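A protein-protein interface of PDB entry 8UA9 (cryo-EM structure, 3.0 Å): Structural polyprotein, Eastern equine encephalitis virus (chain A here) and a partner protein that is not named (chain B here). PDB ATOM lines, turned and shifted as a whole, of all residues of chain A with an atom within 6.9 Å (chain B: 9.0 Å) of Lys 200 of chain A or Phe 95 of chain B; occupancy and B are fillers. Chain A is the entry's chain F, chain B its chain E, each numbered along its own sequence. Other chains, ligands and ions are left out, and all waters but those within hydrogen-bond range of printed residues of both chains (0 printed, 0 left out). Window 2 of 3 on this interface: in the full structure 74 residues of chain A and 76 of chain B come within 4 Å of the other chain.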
ATOM      1  N   TYR A 198      -8.503 -27.099  -1.214  1.00  0.00           N
ATOM      2  CA  TYR A 198      -8.983 -26.321  -0.082  1.00  0.00           C
ATOM      3  C   TYR A 198      -9.151 -27.335   1.028  1.00  0.00           C
ATOM      4  O   TYR A 198     -10.094 -28.134   1.016  1.00  0.00           O
ATOM      5  CB  TYR A 198     -10.278 -25.601  -0.367  1.00  0.00           C
ATOM      6  CG  TYR A 198     -10.727 -24.694   0.746  1.00  0.00           C
ATOM      7  CD1 TYR A 198     -10.274 -23.400   0.839  1.00  0.00           C
ATOM      8  CD2 TYR A 198     -11.619 -25.133   1.693  1.00  0.00           C
ATOM      9  CE1 TYR A 198     -10.692 -22.580   1.846  1.00  0.00           C
ATOM     10  CE2 TYR A 198     -12.046 -24.314   2.701  1.00  0.00           C
ATOM     11  CZ  TYR A 198     -11.581 -23.041   2.771  1.00  0.00           C
ATOM     12  OH  TYR A 198     -12.002 -22.221   3.783  1.00  0.00           O
ATOM     13  N   CYS A 199      -8.198 -27.325   1.948  1.00  0.00           N
ATOM     14  CA  CYS A 199      -8.032 -28.351   2.957  1.00  0.00           C
ATOM     15  C   CYS A 199      -8.191 -27.678   4.300  1.00  0.00           C
ATOM     16  O   CYS A 199      -7.302 -26.944   4.734  1.00  0.00           O
ATOM     17  CB  CYS A 199      -6.649 -28.967   2.830  1.00  0.00           C
ATOM     18  SG  CYS A 199      -6.547 -30.285   1.656  1.00  0.00           S
ATOM     19  N   LYS A 200      -9.313 -27.919   4.954  1.00  0.00           N
ATOM     20  CA  LYS A 200      -9.520 -27.446   6.316  1.00  0.00           C
ATOM     21  C   LYS A 200      -9.155 -28.558   7.298  1.00  0.00           C
ATOM     22  O   LYS A 200      -9.978 -29.139   8.001  1.00  0.00           O
ATOM     23  CB  LYS A 200     -10.923 -26.914   6.513  1.00  0.00           C
ATOM     24  CG  LYS A 200     -11.252 -26.549   7.952  1.00  0.00           C
ATOM     25  CD  LYS A 200     -12.161 -25.340   8.018  1.00  0.00           C
ATOM     26  CE  LYS A 200     -12.552 -25.019   9.449  1.00  0.00           C
ATOM     27  NZ  LYS A 200     -12.855 -23.575   9.639  1.00  0.00           N
ATOM     28  N   CYS A 201      -7.854 -28.835   7.314  1.00  0.00           N
ATOM     29  CA  CYS A 201      -7.251 -29.232   8.559  1.00  0.00           C
ATOM     30  C   CYS A 201      -7.344 -27.953   9.368  1.00  0.00           C
ATOM     31  O   CYS A 201      -7.491 -26.893   8.775  1.00  0.00           O
ATOM     32  CB  CYS A 201      -5.772 -29.561   8.395  1.00  0.00           C
ATOM     33  SG  CYS A 201      -5.178 -30.573   7.016  1.00  0.00           S
ATOM     34  N   PRO A 202      -7.357 -28.013  10.698  1.00  0.00           N
ATOM     35  CA  PRO A 202      -7.931 -26.880  11.459  1.00  0.00           C
ATOM     36  C   PRO A 202      -7.394 -25.503  11.078  1.00  0.00           C
ATOM     37  O   PRO A 202      -8.163 -24.537  11.089  1.00  0.00           O
ATOM     38  CB  PRO A 202      -7.607 -27.227  12.913  1.00  0.00           C
ATOM     39  CG  PRO A 202      -7.197 -28.643  12.934  1.00  0.00           C
ATOM     40  CD  PRO A 202      -7.027 -29.160  11.551  1.00  0.00           C
ATOM     41  N   ASP A 203      -6.113 -25.378  10.724  1.00  0.00           N
ATOM     42  CA  ASP A 203      -5.666 -24.227   9.941  1.00  0.00           C
ATOM     43  C   ASP A 203      -6.151 -24.298   8.497  1.00  0.00           C
ATOM     44  O   ASP A 203      -5.901 -25.279   7.797  1.00  0.00           O
ATOM     45  CB  ASP A 203      -4.140 -24.133   9.960  1.00  0.00           C
ATOM     46  CG  ASP A 203      -3.550 -24.373  11.338  1.00  0.00           C
ATOM     47  OD1 ASP A 203      -3.552 -25.536  11.792  1.00  0.00           O
ATOM     48  OD2 ASP A 203      -3.085 -23.398  11.965  1.00  0.00           O
ATOM     49  N   VAL A 204      -6.627 -23.176   7.974  1.00  0.00           N
ATOM     50  CA  VAL A 204      -7.180 -23.150   6.620  1.00  0.00           C
ATOM     51  C   VAL A 204      -6.031 -23.259   5.623  1.00  0.00           C
ATOM     52  O   VAL A 204      -5.249 -22.320   5.466  1.00  0.00           O
ATOM     53  CB  VAL A 204      -8.004 -21.884   6.381  1.00  0.00           C
ATOM     54  CG1 VAL A 204      -8.267 -21.674   4.903  1.00  0.00           C
ATOM     55  CG2 VAL A 204      -9.315 -21.955   7.150  1.00  0.00           C
ATOM     56  N   ARG A 205      -5.950 -24.384   4.922  1.00  0.00           N
ATOM     57  CA  ARG A 205      -4.881 -24.674   3.978  1.00  0.00           C
ATOM     58  C   ARG A 205      -5.457 -24.655   2.574  1.00  0.00           C
ATOM     59  O   ARG A 205      -6.592 -25.073   2.364  1.00  0.00           O
ATOM     60  CB  ARG A 205      -4.257 -26.043   4.239  1.00  0.00           C
ATOM     61  CG  ARG A 205      -3.587 -26.197   5.581  1.00  0.00           C
ATOM     62  CD  ARG A 205      -2.324 -27.031   5.461  1.00  0.00           C
ATOM     63  NE  ARG A 205      -1.634 -27.173   6.737  1.00  0.00           N
ATOM     64  CZ  ARG A 205      -0.397 -27.630   6.882  1.00  0.00           C
ATOM     65  NH1 ARG A 205       0.330 -28.018   5.844  1.00  0.00           N
ATOM     66  NH2 ARG A 205       0.127 -27.703   8.103  1.00  0.00           N
ATOM     67  N   LYS A 206      -4.707 -24.121   1.618  1.00  0.00           N
ATOM     68  CA  LYS A 206      -5.243 -24.010   0.273  1.00  0.00           C
ATOM     69  C   LYS A 206      -4.120 -23.732  -0.702  1.00  0.00           C
ATOM     70  O   LYS A 206      -3.024 -23.329  -0.315  1.00  0.00           O
ATOM     71  CB  LYS A 206      -6.310 -22.918   0.174  1.00  0.00           C
ATOM     72  CG  LYS A 206      -5.804 -21.507   0.312  1.00  0.00           C
ATOM     73  CD  LYS A 206      -6.951 -20.533   0.267  1.00  0.00           C
ATOM     74  CE  LYS A 206      -6.474 -19.106   0.429  1.00  0.00           C
ATOM     75  NZ  LYS A 206      -6.525 -18.660   1.849  1.00  0.00           N
ATOM     76  N   CYS A 217      -3.598 -33.183   6.763  1.00  0.00           N
ATOM     77  CA  CYS A 217      -4.968 -33.612   7.053  1.00  0.00           C
ATOM     78  C   CYS A 217      -5.068 -35.112   7.288  1.00  0.00           C
ATOM     79  O   CYS A 217      -4.134 -35.868   7.009  1.00  0.00           O
ATOM     80  CB  CYS A 217      -5.954 -33.167   5.969  1.00  0.00           C
ATOM     81  SG  CYS A 217      -6.655 -31.531   6.284  1.00  0.00           S
ATOM     82  N   LYS A 221     -12.565 -36.360   3.674  1.00  0.00           N
ATOM     83  CA  LYS A 221     -13.587 -35.318   3.625  1.00  0.00           C
ATOM     84  C   LYS A 221     -13.214 -34.120   4.486  1.00  0.00           C
ATOM     85  O   LYS A 221     -13.973 -33.636   5.315  1.00  0.00           O
ATOM     86  CB  LYS A 221     -14.935 -35.909   4.026  1.00  0.00           C
ATOM     87  CG  LYS A 221     -15.118 -36.243   5.497  1.00  0.00           C
ATOM     88  CD  LYS A 221     -16.107 -37.377   5.707  1.00  0.00           C
ATOM     89  CE  LYS A 221     -16.931 -37.165   6.971  1.00  0.00           C
ATOM     90  NZ  LYS A 221     -17.964 -38.221   7.158  1.00  0.00           N
ATOM     91  N   GLN A 222     -12.036 -33.593   4.230  1.00  0.00           N
ATOM     92  CA  GLN A 222     -11.671 -32.265   4.669  1.00  0.00           C
ATOM     93  C   GLN A 222     -10.974 -31.468   3.581  1.00  0.00           C
ATOM     94  O   GLN A 222     -10.622 -30.313   3.822  1.00  0.00           O
ATOM     95  CB  GLN A 222     -10.757 -32.323   5.899  1.00  0.00           C
ATOM     96  CG  GLN A 222     -11.216 -33.245   7.035  1.00  0.00           C
ATOM     97  CD  GLN A 222     -10.180 -33.477   8.151  1.00  0.00           C
ATOM     98  OE1 GLN A 222     -10.489 -34.155   9.125  1.00  0.00           O
ATOM     99  NE2 GLN A 222      -8.973 -32.914   8.029  1.00  0.00           N
ATOM    100  N   CYS A 223     -10.757 -32.043   2.406  1.00  0.00           N
ATOM    101  CA  CYS A 223      -9.678 -31.660   1.515  1.00  0.00           C
ATOM    102  C   CYS A 223     -10.173 -31.401   0.101  1.00  0.00           C
ATOM    103  O   CYS A 223      -9.559 -31.817  -0.881  1.00  0.00           O
ATOM    104  CB  CYS A 223      -8.581 -32.701   1.613  1.00  0.00           C
ATOM    105  SG  CYS A 223      -7.320 -32.115   2.742  1.00  0.00           S
ATOM    106  N   ARG A 224     -11.272 -30.663  -0.012  1.00  0.00           N
ATOM    107  CA  ARG A 224     -11.991 -30.515  -1.275  1.00  0.00           C
ATOM    108  C   ARG A 224     -11.097 -30.021  -2.399  1.00  0.00           C
ATOM    109  O   ARG A 224     -10.448 -28.981  -2.275  1.00  0.00           O
ATOM    110  CB  ARG A 224     -13.142 -29.543  -1.096  1.00  0.00           C
ATOM    111  CG  ARG A 224     -14.115 -29.949  -0.037  1.00  0.00           C
ATOM    112  CD  ARG A 224     -15.413 -30.307  -0.596  1.00  0.00           C
ATOM    113  NE  ARG A 224     -16.403 -30.470   0.458  1.00  0.00           N
ATOM    114  CZ  ARG A 224     -16.439 -31.480   1.311  1.00  0.00           C
ATOM    115  NH1 ARG A 224     -15.577 -32.477   1.249  1.00  0.00           N
ATOM    116  NH2 ARG A 224     -17.378 -31.496   2.248  1.00  0.00           N
ATOM    117  N   TYR A 226     -10.467 -29.291  -6.692  1.00  0.00           N
ATOM    118  CA  TYR A 226     -11.130 -28.771  -7.871  1.00  0.00           C
ATOM    119  C   TYR A 226     -10.183 -28.881  -9.047  1.00  0.00           C
ATOM    120  O   TYR A 226      -9.078 -28.340  -9.007  1.00  0.00           O
ATOM    121  CB  TYR A 226     -11.510 -27.315  -7.660  1.00  0.00           C
ATOM    122  CG  TYR A 226     -12.367 -27.074  -6.466  1.00  0.00           C
ATOM    123  CD1 TYR A 226     -13.602 -27.646  -6.376  1.00  0.00           C
ATOM    124  CD2 TYR A 226     -11.950 -26.264  -5.444  1.00  0.00           C
ATOM    125  CE1 TYR A 226     -14.388 -27.433  -5.313  1.00  0.00           C
ATOM    126  CE2 TYR A 226     -12.741 -26.039  -4.366  1.00  0.00           C
ATOM    127  CZ  TYR A 226     -13.959 -26.627  -4.304  1.00  0.00           C
ATOM    128  OH  TYR A 226     -14.765 -26.412  -3.219  1.00  0.00           O
ATOM    129  N   VAL B  60     -20.545 -19.250  -7.562  1.00  0.00           N
ATOM    130  CA  VAL B  60     -20.580 -19.903  -6.259  1.00  0.00           C
ATOM    131  C   VAL B  60     -19.294 -19.577  -5.517  1.00  0.00           C
ATOM    132  O   VAL B  60     -18.220 -20.044  -5.901  1.00  0.00           O
ATOM    133  CB  VAL B  60     -20.748 -21.415  -6.412  1.00  0.00           C
ATOM    134  CG1 VAL B  60     -20.695 -22.066  -5.074  1.00  0.00           C
ATOM    135  CG2 VAL B  60     -22.048 -21.733  -7.086  1.00  0.00           C
ATOM    136  N   LYS B  61     -19.389 -18.772  -4.460  1.00  0.00           N
ATOM    137  CA  LYS B  61     -18.296 -18.547  -3.518  1.00  0.00           C
ATOM    138  C   LYS B  61     -18.422 -19.456  -2.303  1.00  0.00           C
ATOM    139  O   LYS B  61     -19.465 -19.463  -1.636  1.00  0.00           O
ATOM    140  CB  LYS B  61     -18.224 -17.094  -3.078  1.00  0.00           C
ATOM    141  CG  LYS B  61     -17.049 -16.848  -2.178  1.00  0.00           C
ATOM    142  CD  LYS B  61     -16.381 -15.505  -2.416  1.00  0.00           C
ATOM    143  CE  LYS B  61     -15.274 -15.543  -3.459  1.00  0.00           C
ATOM    144  NZ  LYS B  61     -14.260 -16.622  -3.307  1.00  0.00           N
ATOM    145  N   CYS B  62     -17.362 -20.219  -2.021  1.00  0.00           N
ATOM    146  CA  CYS B  62     -17.433 -21.252  -0.994  1.00  0.00           C
ATOM    147  C   CYS B  62     -17.591 -20.709   0.418  1.00  0.00           C
ATOM    148  O   CYS B  62     -18.565 -21.037   1.098  1.00  0.00           O
ATOM    149  CB  CYS B  62     -16.195 -22.133  -1.072  1.00  0.00           C
ATOM    150  SG  CYS B  62     -16.100 -23.164  -2.532  1.00  0.00           S
ATOM    151  N   CYS B  63     -16.670 -19.871   0.884  1.00  0.00           N
ATOM    152  CA  CYS B  63     -16.696 -19.426   2.274  1.00  0.00           C
ATOM    153  C   CYS B  63     -16.851 -17.917   2.356  1.00  0.00           C
ATOM    154  O   CYS B  63     -16.403 -17.279   3.310  1.00  0.00           O
ATOM    155  CB  CYS B  63     -15.437 -19.909   2.995  1.00  0.00           C
ATOM    156  SG  CYS B  63     -15.645 -21.475   3.870  1.00  0.00           S
ATOM    157  N   VAL B  84     -26.173 -22.116   0.540  1.00  0.00           N
ATOM    158  CA  VAL B  84     -26.270 -23.121  -0.506  1.00  0.00           C
ATOM    159  C   VAL B  84     -25.153 -24.131  -0.331  1.00  0.00           C
ATOM    160  O   VAL B  84     -23.982 -23.757  -0.304  1.00  0.00           O
ATOM    161  CB  VAL B  84     -26.221 -22.482  -1.905  1.00  0.00           C
ATOM    162  CG1 VAL B  84     -27.388 -21.564  -2.089  1.00  0.00           C
ATOM    163  CG2 VAL B  84     -24.915 -21.743  -2.180  1.00  0.00           C
ATOM    164  N   TYR B  85     -25.495 -25.412  -0.237  1.00  0.00           N
ATOM    165  CA  TYR B  85     -24.461 -26.437  -0.237  1.00  0.00           C
ATOM    166  C   TYR B  85     -24.552 -27.169  -1.571  1.00  0.00           C
ATOM    167  O   TYR B  85     -25.231 -28.190  -1.677  1.00  0.00           O
ATOM    168  CB  TYR B  85     -24.643 -27.360   0.964  1.00  0.00           C
ATOM    169  CG  TYR B  85     -23.513 -28.326   1.191  1.00  0.00           C
ATOM    170  CD1 TYR B  85     -22.238 -27.886   1.430  1.00  0.00           C
ATOM    171  CD2 TYR B  85     -23.731 -29.675   1.180  1.00  0.00           C
ATOM    172  CE1 TYR B  85     -21.226 -28.750   1.616  1.00  0.00           C
ATOM    173  CE2 TYR B  85     -22.717 -30.544   1.374  1.00  0.00           C
ATOM    174  CZ  TYR B  85     -21.466 -30.075   1.595  1.00  0.00           C
ATOM    175  OH  TYR B  85     -20.434 -30.953   1.800  1.00  0.00           O
ATOM    176  N   PRO B  86     -23.920 -26.643  -2.615  1.00  0.00           N
ATOM    177  CA  PRO B  86     -23.952 -27.284  -3.928  1.00  0.00           C
ATOM    178  C   PRO B  86     -23.347 -28.676  -3.999  1.00  0.00           C
ATOM    179  O   PRO B  86     -22.279 -28.946  -3.453  1.00  0.00           O
ATOM    180  CB  PRO B  86     -23.196 -26.299  -4.813  1.00  0.00           C
ATOM    181  CG  PRO B  86     -22.553 -25.394  -3.953  1.00  0.00           C
ATOM    182  CD  PRO B  86     -23.321 -25.310  -2.724  1.00  0.00           C
ATOM    183  N   ALA B  92     -19.060 -32.553  -3.766  1.00  0.00           N
ATOM    184  CA  ALA B  92     -19.060 -31.837  -2.501  1.00  0.00           C
ATOM    185  C   ALA B  92     -18.725 -30.387  -2.690  1.00  0.00           C
ATOM    186  O   ALA B  92     -17.999 -29.816  -1.881  1.00  0.00           O
ATOM    187  CB  ALA B  92     -18.088 -32.494  -1.528  1.00  0.00           C
ATOM    188  N   TYR B  93     -19.329 -29.743  -3.684  1.00  0.00           N
ATOM    189  CA  TYR B  93     -18.726 -28.619  -4.397  1.00  0.00           C
ATOM    190  C   TYR B  93     -18.012 -27.608  -3.525  1.00  0.00           C
ATOM    191  O   TYR B  93     -16.961 -27.115  -3.926  1.00  0.00           O
ATOM    192  CB  TYR B  93     -19.737 -27.854  -5.241  1.00  0.00           C
ATOM    193  CG  TYR B  93     -19.027 -26.815  -6.069  1.00  0.00           C
ATOM    194  CD1 TYR B  93     -18.228 -27.180  -7.121  1.00  0.00           C
ATOM    195  CD2 TYR B  93     -19.097 -25.485  -5.758  1.00  0.00           C
ATOM    196  CE1 TYR B  93     -17.562 -26.258  -7.848  1.00  0.00           C
ATOM    197  CE2 TYR B  93     -18.421 -24.560  -6.483  1.00  0.00           C
ATOM    198  CZ  TYR B  93     -17.655 -24.955  -7.523  1.00  0.00           C
ATOM    199  OH  TYR B  93     -16.979 -24.030  -8.263  1.00  0.00           O
ATOM    200  N   CYS B  94     -18.552 -27.262  -2.364  1.00  0.00           N
ATOM    201  CA  CYS B  94     -17.912 -26.261  -1.533  1.00  0.00           C
ATOM    202  C   CYS B  94     -17.802 -26.794  -0.113  1.00  0.00           C
ATOM    203  O   CYS B  94     -18.650 -27.563   0.337  1.00  0.00           O
ATOM    204  CB  CYS B  94     -18.739 -25.000  -1.576  1.00  0.00           C
ATOM    205  SG  CYS B  94     -18.287 -23.864  -2.897  1.00  0.00           S
ATOM    206  N   PHE B  95     -16.743 -26.379   0.595  1.00  0.00           N
ATOM    207  CA  PHE B  95     -16.459 -26.972   1.900  1.00  0.00           C
ATOM    208  C   PHE B  95     -17.460 -26.535   2.957  1.00  0.00           C
ATOM    209  O   PHE B  95     -18.114 -27.360   3.599  1.00  0.00           O
ATOM    210  CB  PHE B  95     -15.045 -26.607   2.348  1.00  0.00           C
ATOM    211  CG  PHE B  95     -14.605 -27.342   3.574  1.00  0.00           C
ATOM    212  CD1 PHE B  95     -15.008 -26.964   4.842  1.00  0.00           C
ATOM    213  CD2 PHE B  95     -13.845 -28.465   3.449  1.00  0.00           C
ATOM    214  CE1 PHE B  95     -14.638 -27.668   5.931  1.00  0.00           C
ATOM    215  CE2 PHE B  95     -13.473 -29.163   4.535  1.00  0.00           C
ATOM    216  CZ  PHE B  95     -13.882 -28.782   5.780  1.00  0.00           C
ATOM    217  N   CYS B  96     -17.530 -25.242   3.182  1.00  0.00           N
ATOM    218  CA  CYS B  96     -18.259 -24.658   4.294  1.00  0.00           C
ATOM    219  C   CYS B  96     -19.718 -25.077   4.257  1.00  0.00           C
ATOM    220  O   CYS B  96     -20.389 -24.896   3.239  1.00  0.00           O
ATOM    221  CB  CYS B  96     -18.107 -23.144   4.269  1.00  0.00           C
ATOM    222  SG  CYS B  96     -18.060 -22.390   5.891  1.00  0.00           S
ATOM    223  N   ASP B  97     -20.185 -25.714   5.325  1.00  0.00           N
ATOM    224  CA  ASP B  97     -21.531 -26.278   5.334  1.00  0.00           C
ATOM    225  C   ASP B  97     -22.588 -25.222   5.032  1.00  0.00           C
ATOM    226  O   ASP B  97     -23.382 -25.384   4.101  1.00  0.00           O
ATOM    227  CB  ASP B  97     -21.821 -26.928   6.690  1.00  0.00           C
ATOM    228  CG  ASP B  97     -21.705 -28.448   6.677  1.00  0.00           C
ATOM    229  OD1 ASP B  97     -21.376 -29.057   5.637  1.00  0.00           O
ATOM    230  OD2 ASP B  97     -21.956 -29.052   7.740  1.00  0.00           O
ATOM    231  N   THR B  98     -22.633 -24.141   5.816  1.00  0.00           N
ATOM    232  CA  THR B  98     -23.644 -23.102   5.647  1.00  0.00           C
ATOM    233  C   THR B  98     -23.148 -21.768   5.094  1.00  0.00           C
ATOM    234  O   THR B  98     -23.923 -21.081   4.442  1.00  0.00           O
ATOM    235  CB  THR B  98     -24.349 -22.857   6.985  1.00  0.00           C
ATOM    236  OG1 THR B  98     -25.666 -22.346   6.745  1.00  0.00           O
ATOM    237  CG2 THR B  98     -23.563 -21.899   7.900  1.00  0.00           C
ATOM    238  N   GLU B  99     -21.901 -21.358   5.319  1.00  0.00           N
ATOM    239  CA  GLU B  99     -21.443 -20.043   4.862  1.00  0.00           C
ATOM    240  C   GLU B  99     -21.008 -20.070   3.396  1.00  0.00           C
ATOM    241  O   GLU B  99     -19.879 -19.745   3.043  1.00  0.00           O
ATOM    242  CB  GLU B  99     -20.318 -19.542   5.750  1.00  0.00           C
ATOM    243  CG  GLU B  99     -20.061 -18.038   5.668  1.00  0.00           C
ATOM    244  CD  GLU B  99     -19.351 -17.492   6.897  1.00  0.00           C
ATOM    245  OE1 GLU B  99     -18.239 -17.971   7.199  1.00  0.00           O
ATOM    246  OE2 GLU B  99     -19.897 -16.578   7.552  1.00  0.00           O
ATOM    247  N   ASN B 100     -21.938 -20.448   2.537  1.00  0.00           N
ATOM    248  CA  ASN B 100     -21.762 -20.504   1.094  1.00  0.00           C
ATOM    249  C   ASN B 100     -22.709 -19.541   0.413  1.00  0.00           C
ATOM    250  O   ASN B 100     -23.830 -19.333   0.877  1.00  0.00           O
ATOM    251  CB  ASN B 100     -22.029 -21.854   0.571  1.00  0.00           C
ATOM    252  CG  ASN B 100     -21.018 -22.830   0.969  1.00  0.00           C
ATOM    253  OD1 ASN B 100     -20.339 -22.645   1.947  1.00  0.00           O
ATOM    254  ND2 ASN B 100     -20.951 -23.928   0.255  1.00  0.00           N
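The backbone carbonyl oxygen (O) of Cys 62 of chain B lies close to the backbone carbonyl oxygen (O) of Glu 99 of chain B (2.7 Å).
The side-chain sulfur (SG) of Cys 63 of chain B lies close to the side-chain sulfur (SG) of Cys 96 of chain B, 3.3 Å away.
The backbone NH (N) of Tyr 93 of chain B is in hydrogen-bond range of the backbone carbonyl oxygen (O) of Pro 86 of chain B (3.1 Å).
The backbone carbonyl oxygen of Gln 222 of chain A is in hydrogen-bond range of the backbone NH of Lys 200 of chain A (3.0 Å).
The side-chain sulfur (SG) of Cys 199 of chain A is disulfide-bonded to the side-chain sulfur (SG) of Cys 223 of chain A.
The side-chain sulfur of Cys 201 of chain A forms a disulfide with the side-chain sulfur of Cys 217 of chain A.
Phe 95 of chain B touches just these residues of chain A: Tyr 198, Lys 200, Gln 222 and Arg 224.
No residue of chain B comes within 4 Å of Cys 199 of chain A.
Of the printed residues of chain A, Tyr 85 of chain B touches Arg 224.
Printed residues of chain A within 4 Å of Cys 63 of chain B: Tyr 198 (3.7 Å).
Cys 96 of chain B touches none of the printed residues of chain A.
Glu 99 of chain B touches none of the printed residues of chain A.
The nearest residue of chain B that does not touch Lys 200 of chain A is Cys 96 of chain B (6.5 Å).
SG of Cys 62 of chain B sits at hydrogen-bond distance from OH of Tyr 226 of chain A (3.6 Å).
The side-chain sulfur of Cys 63 of chain B lies within hydrogen-bond range of the side-chain hydroxyl of Tyr 198 of chain A (3.7 Å).
The guanidinium group (NH2) of Arg 224 of chain A lies within hydrogen-bond range of the side-chain hydroxyl (OH) of Tyr 85 of chain B (3.1 Å).
The backbone carbonyl oxygen (O) of Ala 92 of chain B sits at hydrogen-bond distance from the guanidinium group (NE) of Arg 224 of chain A, 2.9 Å away.
The backbone carbonyl oxygen (O) of Tyr 93 of chain B sits at hydrogen-bond distance from the side-chain hydroxyl (OH) of Tyr 226 of chain A (2.4 Å).
Of the 16 printed residues of chain B, 7 touch a printed residue of chain A.
Printed residues of chain B that touch a printed residue of chain A: Cys 62, Cys 63, Tyr 85, Ala 92, Tyr 93, Cys 94 and Phe 95.
Hydrophobic or aromatic side chains of chain B within 4 Å of the printed part of chain A: Tyr 85, Ala 92 and Phe 95.
Printed residues of chain A that touch a printed residue of chain B: Tyr 198, Lys 200, Gln 222, Arg 224 and Tyr 226.
Hydrophobic or aromatic side chains of chain A that line the printed part of chain B: Tyr 198 and Tyr 226.
Among the printed residues, 11 pairs touch across the chains.
Among the printed residues, no Asp or Glu carboxylate lies within 4 Å of a Lys or Arg side-chain nitrogen of the other chain.
Among the printed residues, pairs that only touch across the chains: Tyr 198 of chain A with Phe 95 of chain B, Lys 200 of chain A with Phe 95 of chain B, Gln 222 of chain A with Phe 95 of chain B, Arg 224 of chain A with Cys 94 of chain B, Arg 224 of chain A with Phe 95 of chain B and Tyr 226 of chain A with Cys 94 of chain B.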
